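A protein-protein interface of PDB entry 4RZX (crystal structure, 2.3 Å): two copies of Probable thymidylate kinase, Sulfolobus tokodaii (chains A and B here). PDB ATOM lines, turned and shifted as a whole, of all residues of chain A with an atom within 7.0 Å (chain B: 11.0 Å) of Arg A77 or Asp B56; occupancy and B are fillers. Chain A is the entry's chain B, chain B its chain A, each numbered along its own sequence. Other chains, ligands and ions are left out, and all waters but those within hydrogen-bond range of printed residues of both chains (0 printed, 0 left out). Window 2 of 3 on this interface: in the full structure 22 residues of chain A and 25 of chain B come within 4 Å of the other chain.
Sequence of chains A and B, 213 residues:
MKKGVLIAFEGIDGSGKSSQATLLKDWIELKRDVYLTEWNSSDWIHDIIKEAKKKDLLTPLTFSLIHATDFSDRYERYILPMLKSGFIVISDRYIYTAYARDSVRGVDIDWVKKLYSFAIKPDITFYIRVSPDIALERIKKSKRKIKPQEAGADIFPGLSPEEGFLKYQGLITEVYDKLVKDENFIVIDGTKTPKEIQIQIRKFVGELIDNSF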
ATOM      1  N   TYR A  35      27.499  19.181  32.140  1.00  0.00           N
ATOM      2  CA  TYR A  35      26.040  19.198  32.108  1.00  0.00           C
ATOM      3  C   TYR A  35      25.550  18.926  30.685  1.00  0.00           C
ATOM      4  O   TYR A  35      26.112  19.447  29.703  1.00  0.00           O
ATOM      5  CB  TYR A  35      25.564  20.571  32.531  1.00  0.00           C
ATOM      6  CG  TYR A  35      24.101  20.814  32.341  1.00  0.00           C
ATOM      7  CD1 TYR A  35      23.175  20.306  33.252  1.00  0.00           C
ATOM      8  CD2 TYR A  35      23.624  21.560  31.243  1.00  0.00           C
ATOM      9  CE1 TYR A  35      21.819  20.531  33.088  1.00  0.00           C
ATOM     10  CE2 TYR A  35      22.268  21.794  31.082  1.00  0.00           C
ATOM     11  CZ  TYR A  35      21.379  21.280  32.019  1.00  0.00           C
ATOM     12  OH  TYR A  35      20.038  21.493  31.891  1.00  0.00           O
ATOM     13  N   PHE A  71      14.050  27.013  22.867  1.00  0.00           N
ATOM     14  CA  PHE A  71      15.472  27.077  22.928  1.00  0.00           C
ATOM     15  C   PHE A  71      15.935  28.214  23.838  1.00  0.00           C
ATOM     16  O   PHE A  71      16.873  28.029  24.625  1.00  0.00           O
ATOM     17  CB  PHE A  71      16.081  27.287  21.554  1.00  0.00           C
ATOM     18  CG  PHE A  71      17.559  27.394  21.605  1.00  0.00           C
ATOM     19  CD1 PHE A  71      18.337  26.270  21.631  1.00  0.00           C
ATOM     20  CD2 PHE A  71      18.160  28.607  21.723  1.00  0.00           C
ATOM     21  CE1 PHE A  71      19.707  26.361  21.770  1.00  0.00           C
ATOM     22  CE2 PHE A  71      19.521  28.710  21.827  1.00  0.00           C
ATOM     23  CZ  PHE A  71      20.291  27.590  21.873  1.00  0.00           C
ATOM     24  N   SER A  72      15.339  29.404  23.696  1.00  0.00           N
ATOM     25  CA  SER A  72      15.757  30.528  24.529  1.00  0.00           C
ATOM     26  C   SER A  72      15.583  30.231  25.985  1.00  0.00           C
ATOM     27  O   SER A  72      16.345  30.696  26.812  1.00  0.00           O
ATOM     28  CB  SER A  72      14.984  31.839  24.200  1.00  0.00           C
ATOM     29  OG  SER A  72      13.616  31.801  24.564  1.00  0.00           O
ATOM     30  N   ASP A  73      14.541  29.487  26.311  1.00  0.00           N
ATOM     31  CA  ASP A  73      14.248  29.183  27.711  1.00  0.00           C
ATOM     32  C   ASP A  73      15.337  28.296  28.290  1.00  0.00           C
ATOM     33  O   ASP A  73      15.958  28.617  29.282  1.00  0.00           O
ATOM     34  CB  ASP A  73      12.876  28.513  27.863  1.00  0.00           C
ATOM     35  CG  ASP A  73      12.516  28.291  29.300  1.00  0.00           C
ATOM     36  OD1 ASP A  73      12.437  29.283  30.035  1.00  0.00           O
ATOM     37  OD2 ASP A  73      12.361  27.129  29.733  1.00  0.00           O
ATOM     38  N   ARG A  74      15.618  27.213  27.620  1.00  0.00           N
ATOM     39  CA  ARG A  74      16.689  26.324  28.067  1.00  0.00           C
ATOM     40  C   ARG A  74      18.082  27.027  28.051  1.00  0.00           C
ATOM     41  O   ARG A  74      18.923  26.802  28.950  1.00  0.00           O
ATOM     42  CB  ARG A  74      16.631  24.981  27.278  1.00  0.00           C
ATOM     43  CG  ARG A  74      17.602  24.817  26.126  1.00  0.00           C
ATOM     44  CD  ARG A  74      17.176  23.680  25.194  1.00  0.00           C
ATOM     45  NE  ARG A  74      18.311  22.960  24.607  1.00  0.00           N
ATOM     46  CZ  ARG A  74      18.377  22.523  23.349  1.00  0.00           C
ATOM     47  NH1 ARG A  74      17.381  22.749  22.488  1.00  0.00           N
ATOM     48  NH2 ARG A  74      19.467  21.874  22.936  1.00  0.00           N
ATOM     49  N   TYR A  75      18.300  27.901  27.071  1.00  0.00           N
ATOM     50  CA  TYR A  75      19.588  28.563  26.917  1.00  0.00           C
ATOM     51  C   TYR A  75      19.799  29.471  28.116  1.00  0.00           C
ATOM     52  O   TYR A  75      20.795  29.376  28.796  1.00  0.00           O
ATOM     53  CB  TYR A  75      19.689  29.361  25.583  1.00  0.00           C
ATOM     54  CG  TYR A  75      21.046  30.107  25.397  1.00  0.00           C
ATOM     55  CD1 TYR A  75      22.180  29.435  24.910  1.00  0.00           C
ATOM     56  CD2 TYR A  75      21.202  31.444  25.797  1.00  0.00           C
ATOM     57  CE1 TYR A  75      23.402  30.088  24.785  1.00  0.00           C
ATOM     58  CE2 TYR A  75      22.420  32.117  25.640  1.00  0.00           C
ATOM     59  CZ  TYR A  75      23.504  31.416  25.147  1.00  0.00           C
ATOM     60  OH  TYR A  75      24.677  32.036  25.016  1.00  0.00           O
ATOM     61  N   GLU A  76      18.848  30.327  28.416  1.00  0.00           N
ATOM     62  CA  GLU A  76      19.066  31.294  29.493  1.00  0.00           C
ATOM     63  C   GLU A  76      18.872  30.688  30.872  1.00  0.00           C
ATOM     64  O   GLU A  76      19.417  31.177  31.840  1.00  0.00           O
ATOM     65  CB  GLU A  76      18.204  32.536  29.289  1.00  0.00           C
ATOM     66  CG  GLU A  76      18.638  33.371  28.079  1.00  0.00           C
ATOM     67  CD  GLU A  76      18.171  34.819  28.128  1.00  0.00           C
ATOM     68  OE1 GLU A  76      17.007  35.050  28.512  1.00  0.00           O
ATOM     69  OE2 GLU A  76      18.961  35.726  27.756  1.00  0.00           O
ATOM     70  N   ARG A  77      18.186  29.565  30.977  1.00  0.00           N
ATOM     71  CA  ARG A  77      17.987  28.995  32.307  1.00  0.00           C
ATOM     72  C   ARG A  77      18.937  27.838  32.631  1.00  0.00           C
ATOM     73  O   ARG A  77      19.256  27.609  33.788  1.00  0.00           O
ATOM     74  CB  ARG A  77      16.514  28.649  32.495  1.00  0.00           C
ATOM     75  CG  ARG A  77      15.583  29.868  32.249  1.00  0.00           C
ATOM     76  CD  ARG A  77      14.643  30.157  33.437  1.00  0.00           C
ATOM     77  NE  ARG A  77      14.303  28.926  34.182  1.00  0.00           N
ATOM     78  CZ  ARG A  77      13.389  28.031  33.814  1.00  0.00           C
ATOM     79  NH1 ARG A  77      12.637  28.215  32.727  1.00  0.00           N
ATOM     80  NH2 ARG A  77      13.206  26.953  34.562  1.00  0.00           N
ATOM     81  N   TYR A  78      19.419  27.120  31.628  1.00  0.00           N
ATOM     82  CA  TYR A  78      20.380  26.051  31.903  1.00  0.00           C
ATOM     83  C   TYR A  78      21.745  26.251  31.218  1.00  0.00           C
ATOM     84  O   TYR A  78      22.779  26.219  31.872  1.00  0.00           O
ATOM     85  CB  TYR A  78      19.779  24.680  31.586  1.00  0.00           C
ATOM     86  CG  TYR A  78      18.502  24.385  32.362  1.00  0.00           C
ATOM     87  CD1 TYR A  78      17.274  24.860  31.922  1.00  0.00           C
ATOM     88  CD2 TYR A  78      18.523  23.630  33.550  1.00  0.00           C
ATOM     89  CE1 TYR A  78      16.102  24.594  32.613  1.00  0.00           C
ATOM     90  CE2 TYR A  78      17.358  23.354  34.246  1.00  0.00           C
ATOM     91  CZ  TYR A  78      16.145  23.846  33.772  1.00  0.00           C
ATOM     92  OH  TYR A  78      14.960  23.604  34.446  1.00  0.00           O
ATOM     93  N   ILE A  79      21.769  26.476  29.919  1.00  0.00           N
ATOM     94  CA  ILE A  79      23.025  26.411  29.212  1.00  0.00           C
ATOM     95  C   ILE A  79      23.963  27.505  29.711  1.00  0.00           C
ATOM     96  O   ILE A  79      25.062  27.210  30.154  1.00  0.00           O
ATOM     97  CB  ILE A  79      22.858  26.547  27.708  1.00  0.00           C
ATOM     98  CG1 ILE A  79      22.028  25.413  27.185  1.00  0.00           C
ATOM     99  CG2 ILE A  79      24.227  26.517  27.020  1.00  0.00           C
ATOM    100  CD1 ILE A  79      21.734  25.564  25.722  1.00  0.00           C
ATOM    101  N   LEU A  80      23.510  28.750  29.654  1.00  0.00           N
ATOM    102  CA  LEU A  80      24.343  29.902  29.984  1.00  0.00           C
ATOM    103  C   LEU A  80      24.762  29.952  31.438  1.00  0.00           C
ATOM    104  O   LEU A  80      25.954  30.089  31.720  1.00  0.00           O
ATOM    105  CB  LEU A  80      23.704  31.228  29.502  1.00  0.00           C
ATOM    106  CG  LEU A  80      24.692  32.392  29.285  1.00  0.00           C
ATOM    107  CD1 LEU A  80      25.707  32.021  28.222  1.00  0.00           C
ATOM    108  CD2 LEU A  80      24.086  33.760  28.918  1.00  0.00           C
ATOM    109  N   PRO A  81      23.830  29.788  32.386  1.00  0.00           N
ATOM    110  CA  PRO A  81      24.317  29.769  33.782  1.00  0.00           C
ATOM    111  C   PRO A  81      25.404  28.727  34.109  1.00  0.00           C
ATOM    112  O   PRO A  81      26.313  29.035  34.873  1.00  0.00           O
ATOM    113  CB  PRO A  81      23.055  29.468  34.588  1.00  0.00           C
ATOM    114  CG  PRO A  81      21.951  30.004  33.757  1.00  0.00           C
ATOM    115  CD  PRO A  81      22.357  29.745  32.327  1.00  0.00           C
ATOM    116  N   MET A  82      25.322  27.509  33.571  1.00  0.00           N
ATOM    117  CA  MET A  82      26.311  26.468  33.921  1.00  0.00           C
ATOM    118  C   MET A  82      27.650  26.760  33.265  1.00  0.00           C
ATOM    119  O   MET A  82      28.706  26.475  33.833  1.00  0.00           O
ATOM    120  CB  MET A  82      25.842  25.058  33.512  1.00  0.00           C
ATOM    121  CG  MET A  82      24.504  24.621  34.096  1.00  0.00           C
ATOM    122  SD  MET A  82      24.695  23.825  35.674  1.00  0.00           S
ATOM    123  CE  MET A  82      23.052  23.151  35.859  1.00  0.00           C
ATOM    124  N   ILE B  48      -1.065  28.962  26.027  1.00  0.00           N
ATOM    125  CA  ILE B  48      -0.555  27.613  26.399  1.00  0.00           C
ATOM    126  C   ILE B  48       0.832  27.710  27.017  1.00  0.00           C
ATOM    127  O   ILE B  48       1.138  26.985  27.940  1.00  0.00           O
ATOM    128  CB  ILE B  48      -0.505  26.680  25.185  1.00  0.00           C
ATOM    129  CG1 ILE B  48      -1.935  26.283  24.808  1.00  0.00           C
ATOM    130  CG2 ILE B  48       0.363  25.426  25.420  1.00  0.00           C
ATOM    131  CD1 ILE B  48      -2.088  25.769  23.396  1.00  0.00           C
ATOM    132  N   ILE B  49       1.666  28.602  26.505  1.00  0.00           N
ATOM    133  CA  ILE B  49       3.057  28.682  26.914  1.00  0.00           C
ATOM    134  C   ILE B  49       3.135  29.334  28.283  1.00  0.00           C
ATOM    135  O   ILE B  49       3.772  28.812  29.195  1.00  0.00           O
ATOM    136  CB  ILE B  49       3.923  29.452  25.896  1.00  0.00           C
ATOM    137  CG1 ILE B  49       3.948  28.692  24.560  1.00  0.00           C
ATOM    138  CG2 ILE B  49       5.336  29.531  26.417  1.00  0.00           C
ATOM    139  CD1 ILE B  49       4.710  29.377  23.434  1.00  0.00           C
ATOM    140  N   LYS B  50       2.485  30.479  28.429  1.00  0.00           N
ATOM    141  CA  LYS B  50       2.443  31.126  29.712  1.00  0.00           C
ATOM    142  C   LYS B  50       1.869  30.234  30.786  1.00  0.00           C
ATOM    143  O   LYS B  50       2.506  30.100  31.823  1.00  0.00           O
ATOM    144  CB  LYS B  50       1.724  32.448  29.620  1.00  0.00           C
ATOM    145  CG  LYS B  50       2.548  33.501  28.846  1.00  0.00           C
ATOM    146  CD  LYS B  50       2.181  34.898  29.309  1.00  0.00           C
ATOM    147  CE  LYS B  50       2.863  36.032  28.553  1.00  0.00           C
ATOM    148  NZ  LYS B  50       2.319  37.327  29.053  1.00  0.00           N
ATOM    149  N   GLU B  51       0.748  29.540  30.544  1.00  0.00           N
ATOM    150  CA  GLU B  51       0.194  28.680  31.616  1.00  0.00           C
ATOM    151  C   GLU B  51       1.160  27.537  31.938  1.00  0.00           C
ATOM    152  O   GLU B  51       1.450  27.292  33.110  1.00  0.00           O
ATOM    153  CB  GLU B  51      -1.236  28.174  31.334  1.00  0.00           C
ATOM    154  CG  GLU B  51      -1.775  27.189  32.389  1.00  0.00           C
ATOM    155  CD  GLU B  51      -3.180  26.597  32.108  1.00  0.00           C
ATOM    156  OE1 GLU B  51      -3.851  26.987  31.163  1.00  0.00           O
ATOM    157  OE2 GLU B  51      -3.649  25.726  32.850  1.00  0.00           O
ATOM    158  N   ALA B  52       1.685  26.874  30.918  1.00  0.00           N
ATOM    159  CA  ALA B  52       2.630  25.794  31.124  1.00  0.00           C
ATOM    160  C   ALA B  52       3.903  26.193  31.906  1.00  0.00           C
ATOM    161  O   ALA B  52       4.519  25.335  32.571  1.00  0.00           O
ATOM    162  CB  ALA B  52       3.028  25.185  29.811  1.00  0.00           C
ATOM    163  N   LYS B  53       4.283  27.466  31.817  1.00  0.00           N
ATOM    164  CA  LYS B  53       5.492  27.966  32.462  1.00  0.00           C
ATOM    165  C   LYS B  53       5.122  28.851  33.661  1.00  0.00           C
ATOM    166  O   LYS B  53       5.945  29.680  34.092  1.00  0.00           O
ATOM    167  CB  LYS B  53       6.362  28.803  31.469  1.00  0.00           C
ATOM    168  CG  LYS B  53       6.995  28.109  30.246  1.00  0.00           C
ATOM    169  CD  LYS B  53       7.658  26.756  30.514  1.00  0.00           C
ATOM    170  CE  LYS B  53       9.150  26.824  30.851  1.00  0.00           C
ATOM    171  NZ  LYS B  53       9.620  25.421  31.075  1.00  0.00           N
ATOM    172  N   LYS B  54       3.896  28.712  34.178  1.00  0.00           N
ATOM    173  CA  LYS B  54       3.401  29.544  35.306  1.00  0.00           C
ATOM    174  C   LYS B  54       4.291  29.449  36.566  1.00  0.00           C
ATOM    175  O   LYS B  54       4.376  30.406  37.313  1.00  0.00           O
ATOM    176  CB  LYS B  54       1.956  29.178  35.701  1.00  0.00           C
ATOM    177  N   LYS B  55       4.935  28.292  36.767  1.00  0.00           N
ATOM    178  CA  LYS B  55       5.801  28.042  37.912  1.00  0.00           C
ATOM    179  C   LYS B  55       7.148  28.769  37.731  1.00  0.00           C
ATOM    180  O   LYS B  55       7.611  29.448  38.643  1.00  0.00           O
ATOM    181  CB  LYS B  55       5.998  26.523  38.106  1.00  0.00           C
ATOM    182  N   ASP B  56       7.723  28.671  36.523  1.00  0.00           N
ATOM    183  CA  ASP B  56       9.065  29.222  36.217  1.00  0.00           C
ATOM    184  C   ASP B  56       9.053  30.738  36.043  1.00  0.00           C
ATOM    185  O   ASP B  56       8.029  31.331  35.700  1.00  0.00           O
ATOM    186  CB  ASP B  56       9.632  28.573  34.959  1.00  0.00           C
ATOM    187  CG  ASP B  56       9.592  27.044  35.018  1.00  0.00           C
ATOM    188  OD1 ASP B  56      10.181  26.453  35.960  1.00  0.00           O
ATOM    189  OD2 ASP B  56       8.966  26.429  34.118  1.00  0.00           O
ATOM    190  N   LEU B  57      10.190  31.361  36.355  1.00  0.00           N
ATOM    191  CA  LEU B  57      10.448  32.773  36.017  1.00  0.00           C
ATOM    192  C   LEU B  57      11.078  32.881  34.586  1.00  0.00           C
ATOM    193  O   LEU B  57      12.196  32.387  34.317  1.00  0.00           O
ATOM    194  CB  LEU B  57      11.364  33.424  37.065  1.00  0.00           C
ATOM    195  CG  LEU B  57      11.438  34.963  37.010  1.00  0.00           C
ATOM    196  CD1 LEU B  57      10.127  35.629  37.429  1.00  0.00           C
ATOM    197  CD2 LEU B  57      12.567  35.434  37.911  1.00  0.00           C
ATOM    198  N   LEU B  58      10.346  33.508  33.685  1.00  0.00           N
ATOM    199  CA  LEU B  58      10.791  33.651  32.284  1.00  0.00           C
ATOM    200  C   LEU B  58      11.676  34.879  32.151  1.00  0.00           C
ATOM    201  O   LEU B  58      11.415  35.915  32.739  1.00  0.00           O
ATOM    202  CB  LEU B  58       9.599  33.737  31.306  1.00  0.00           C
ATOM    203  CG  LEU B  58       8.591  32.574  31.248  1.00  0.00           C
ATOM    204  CD1 LEU B  58       7.455  32.926  30.316  1.00  0.00           C
ATOM    205  CD2 LEU B  58       9.221  31.251  30.806  1.00  0.00           C
ATOM    206  N   THR B  59      12.744  34.740  31.387  1.00  0.00           N
ATOM    207  CA  THR B  59      13.615  35.868  31.104  1.00  0.00           C
ATOM    208  C   THR B  59      12.964  36.773  30.074  1.00  0.00           C
ATOM    209  O   THR B  59      11.993  36.381  29.438  1.00  0.00           O
ATOM    210  CB  THR B  59      14.916  35.398  30.517  1.00  0.00           C
ATOM    211  OG1 THR B  59      14.634  34.741  29.281  1.00  0.00           O
ATOM    212  CG2 THR B  59      15.642  34.408  31.494  1.00  0.00           C
ATOM    213  N   PRO B  60      13.488  38.000  29.925  1.00  0.00           N
ATOM    214  CA  PRO B  60      12.888  38.922  28.979  1.00  0.00           C
ATOM    215  C   PRO B  60      12.961  38.417  27.537  1.00  0.00           C
ATOM    216  O   PRO B  60      12.044  38.677  26.745  1.00  0.00           O
ATOM    217  CB  PRO B  60      13.707  40.210  29.185  1.00  0.00           C
ATOM    218  CG  PRO B  60      14.141  40.128  30.642  1.00  0.00           C
ATOM    219  CD  PRO B  60      14.484  38.681  30.795  1.00  0.00           C
ATOM    220  N   LEU B  61      14.010  37.687  27.200  1.00  0.00           N
ATOM    221  CA  LEU B  61      14.180  37.246  25.855  1.00  0.00           C
ATOM    222  C   LEU B  61      13.031  36.285  25.519  1.00  0.00           C
ATOM    223  O   LEU B  61      12.352  36.387  24.490  1.00  0.00           O
ATOM    224  CB  LEU B  61      15.569  36.597  25.734  1.00  0.00           C
ATOM    225  CG  LEU B  61      15.919  35.897  24.438  1.00  0.00           C
ATOM    226  CD1 LEU B  61      15.770  36.881  23.292  1.00  0.00           C
ATOM    227  CD2 LEU B  61      17.388  35.437  24.483  1.00  0.00           C
ATOM    228  N   THR B  62      12.790  35.376  26.447  1.00  0.00           N
ATOM    229  CA  THR B  62      11.775  34.340  26.310  1.00  0.00           C
ATOM    230  C   THR B  62      10.363  34.984  26.285  1.00  0.00           C
ATOM    231  O   THR B  62       9.541  34.654  25.448  1.00  0.00           O
ATOM    232  CB  THR B  62      11.929  33.307  27.446  1.00  0.00           C
ATOM    233  OG1 THR B  62      13.172  32.636  27.294  1.00  0.00           O
ATOM    234  CG2 THR B  62      10.832  32.249  27.376  1.00  0.00           C
ATOM    235  N   PHE B  63      10.078  35.877  27.223  1.00  0.00           N
ATOM    236  CA  PHE B  63       8.842  36.674  27.222  1.00  0.00           C
ATOM    237  C   PHE B  63       8.631  37.275  25.827  1.00  0.00           C
ATOM    238  O   PHE B  63       7.575  37.142  25.225  1.00  0.00           O
ATOM    239  CB  PHE B  63       8.980  37.800  28.249  1.00  0.00           C
ATOM    240  CG  PHE B  63       7.715  38.560  28.527  1.00  0.00           C
ATOM    241  CD1 PHE B  63       6.785  38.084  29.442  1.00  0.00           C
ATOM    242  CD2 PHE B  63       7.487  39.789  27.929  1.00  0.00           C
ATOM    243  CE1 PHE B  63       5.628  38.805  29.719  1.00  0.00           C
ATOM    244  CE2 PHE B  63       6.339  40.495  28.201  1.00  0.00           C
ATOM    245  CZ  PHE B  63       5.417  40.008  29.099  1.00  0.00           C
ATOM    246  N   ILE B  66       7.710  34.734  23.139  1.00  0.00           N
ATOM    247  CA  ILE B  66       6.403  34.125  23.299  1.00  0.00           C
ATOM    248  C   ILE B  66       5.429  35.024  22.538  1.00  0.00           C
ATOM    249  O   ILE B  66       4.641  34.581  21.694  1.00  0.00           O
ATOM    250  CB  ILE B  66       6.058  34.030  24.778  1.00  0.00           C
ATOM    251  CG1 ILE B  66       6.847  32.865  25.387  1.00  0.00           C
ATOM    252  CG2 ILE B  66       4.583  33.765  24.995  1.00  0.00           C
ATOM    253  CD1 ILE B  66       6.779  32.841  26.900  1.00  0.00           C
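Of the 13 printed residues of chain A, 4 touch a printed residue of chain B.
Printed residues of chain A that touch a printed residue of chain B: Ser A72, Asp A73, Glu A76 and Arg A77.
Among the printed residues, Asp or Glu carboxylates within 4 Å of a Lys or Arg side-chain nitrogen of the other chain: Asp A73 with Lys B53 (3.5 Å) and Arg A77 with Asp B56 (3.4 Å).
NZ of Lys B53 lies within salt-bridge range of OD2 of Asp B56, 3.3 Å away.
OG1 of Thr B59 lies within hydrogen-bond range of OG1 of Thr B62.
The guanidinium group (NH1) of Arg A77 is in salt-bridge range of the side-chain carboxylate (OD1) of Asp A73, at 2.9 Å.
No position is printed for both chains.
Of the 8 pairs that touch across the chains among the printed residues, none has its exchanged pair printed and touching as well.
Of chain B, only Asp B56 (3.4 Å) and Leu B57 (3.4 Å) come within 4 Å of Arg A77.
Asp B56 touches just one residue of chain A: Arg A77.
Asp A73 touches just these residues of chain B: Lys B53 (3.4 Å), Leu B58 (3.8 Å) and Thr B62 (3.6 Å).
Printed residues of chain A within 4 Å of Leu B57: Arg A77 (3.4 Å).
Printed residues of chain B within 4 Å of Glu A76: Thr B59 (2.5 Å) and Leu B61 (3.5 Å).
Of the printed residues of chain A, Thr B59 touches Glu A76 (2.5 Å).
Of the printed residues of chain A, Leu B58 touches Asp A73.
Printed residues of chain B within 4 Å of Ser A72: Thr B62 (2.9 Å).
The nearest residue of chain A that does not touch Asp B56 is Asp A73 (5.6 Å).
The nearest printed residue of chain B that does not touch Glu A76 is Thr B62 (4.7 Å).
Among the printed residues, pairs that only touch across the chains: Asp A73 with Leu B58, Asp A73 with Thr B62, Glu A76 with Leu B61 and Arg A77 with Leu B57.
The side-chain carboxylate of Asp A73 is in salt-bridge range of the side-chain amino group of Lys B53 (3.5 Å).
The side-chain carboxylate (OD1) of Asp B56 is in salt-bridge range of the guanidinium group (NH2) of Arg A77 (3.4 Å).
The side-chain hydroxyl (OG1) of Thr B59 sits at hydrogen-bond distance from the side-chain carboxylate (OE1) of Glu A76 (2.5 Å).
The side-chain hydroxyl (OG1) of Thr B62 lies within hydrogen-bond range of the side-chain hydroxyl (OG) of Ser A72 (2.9 Å).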
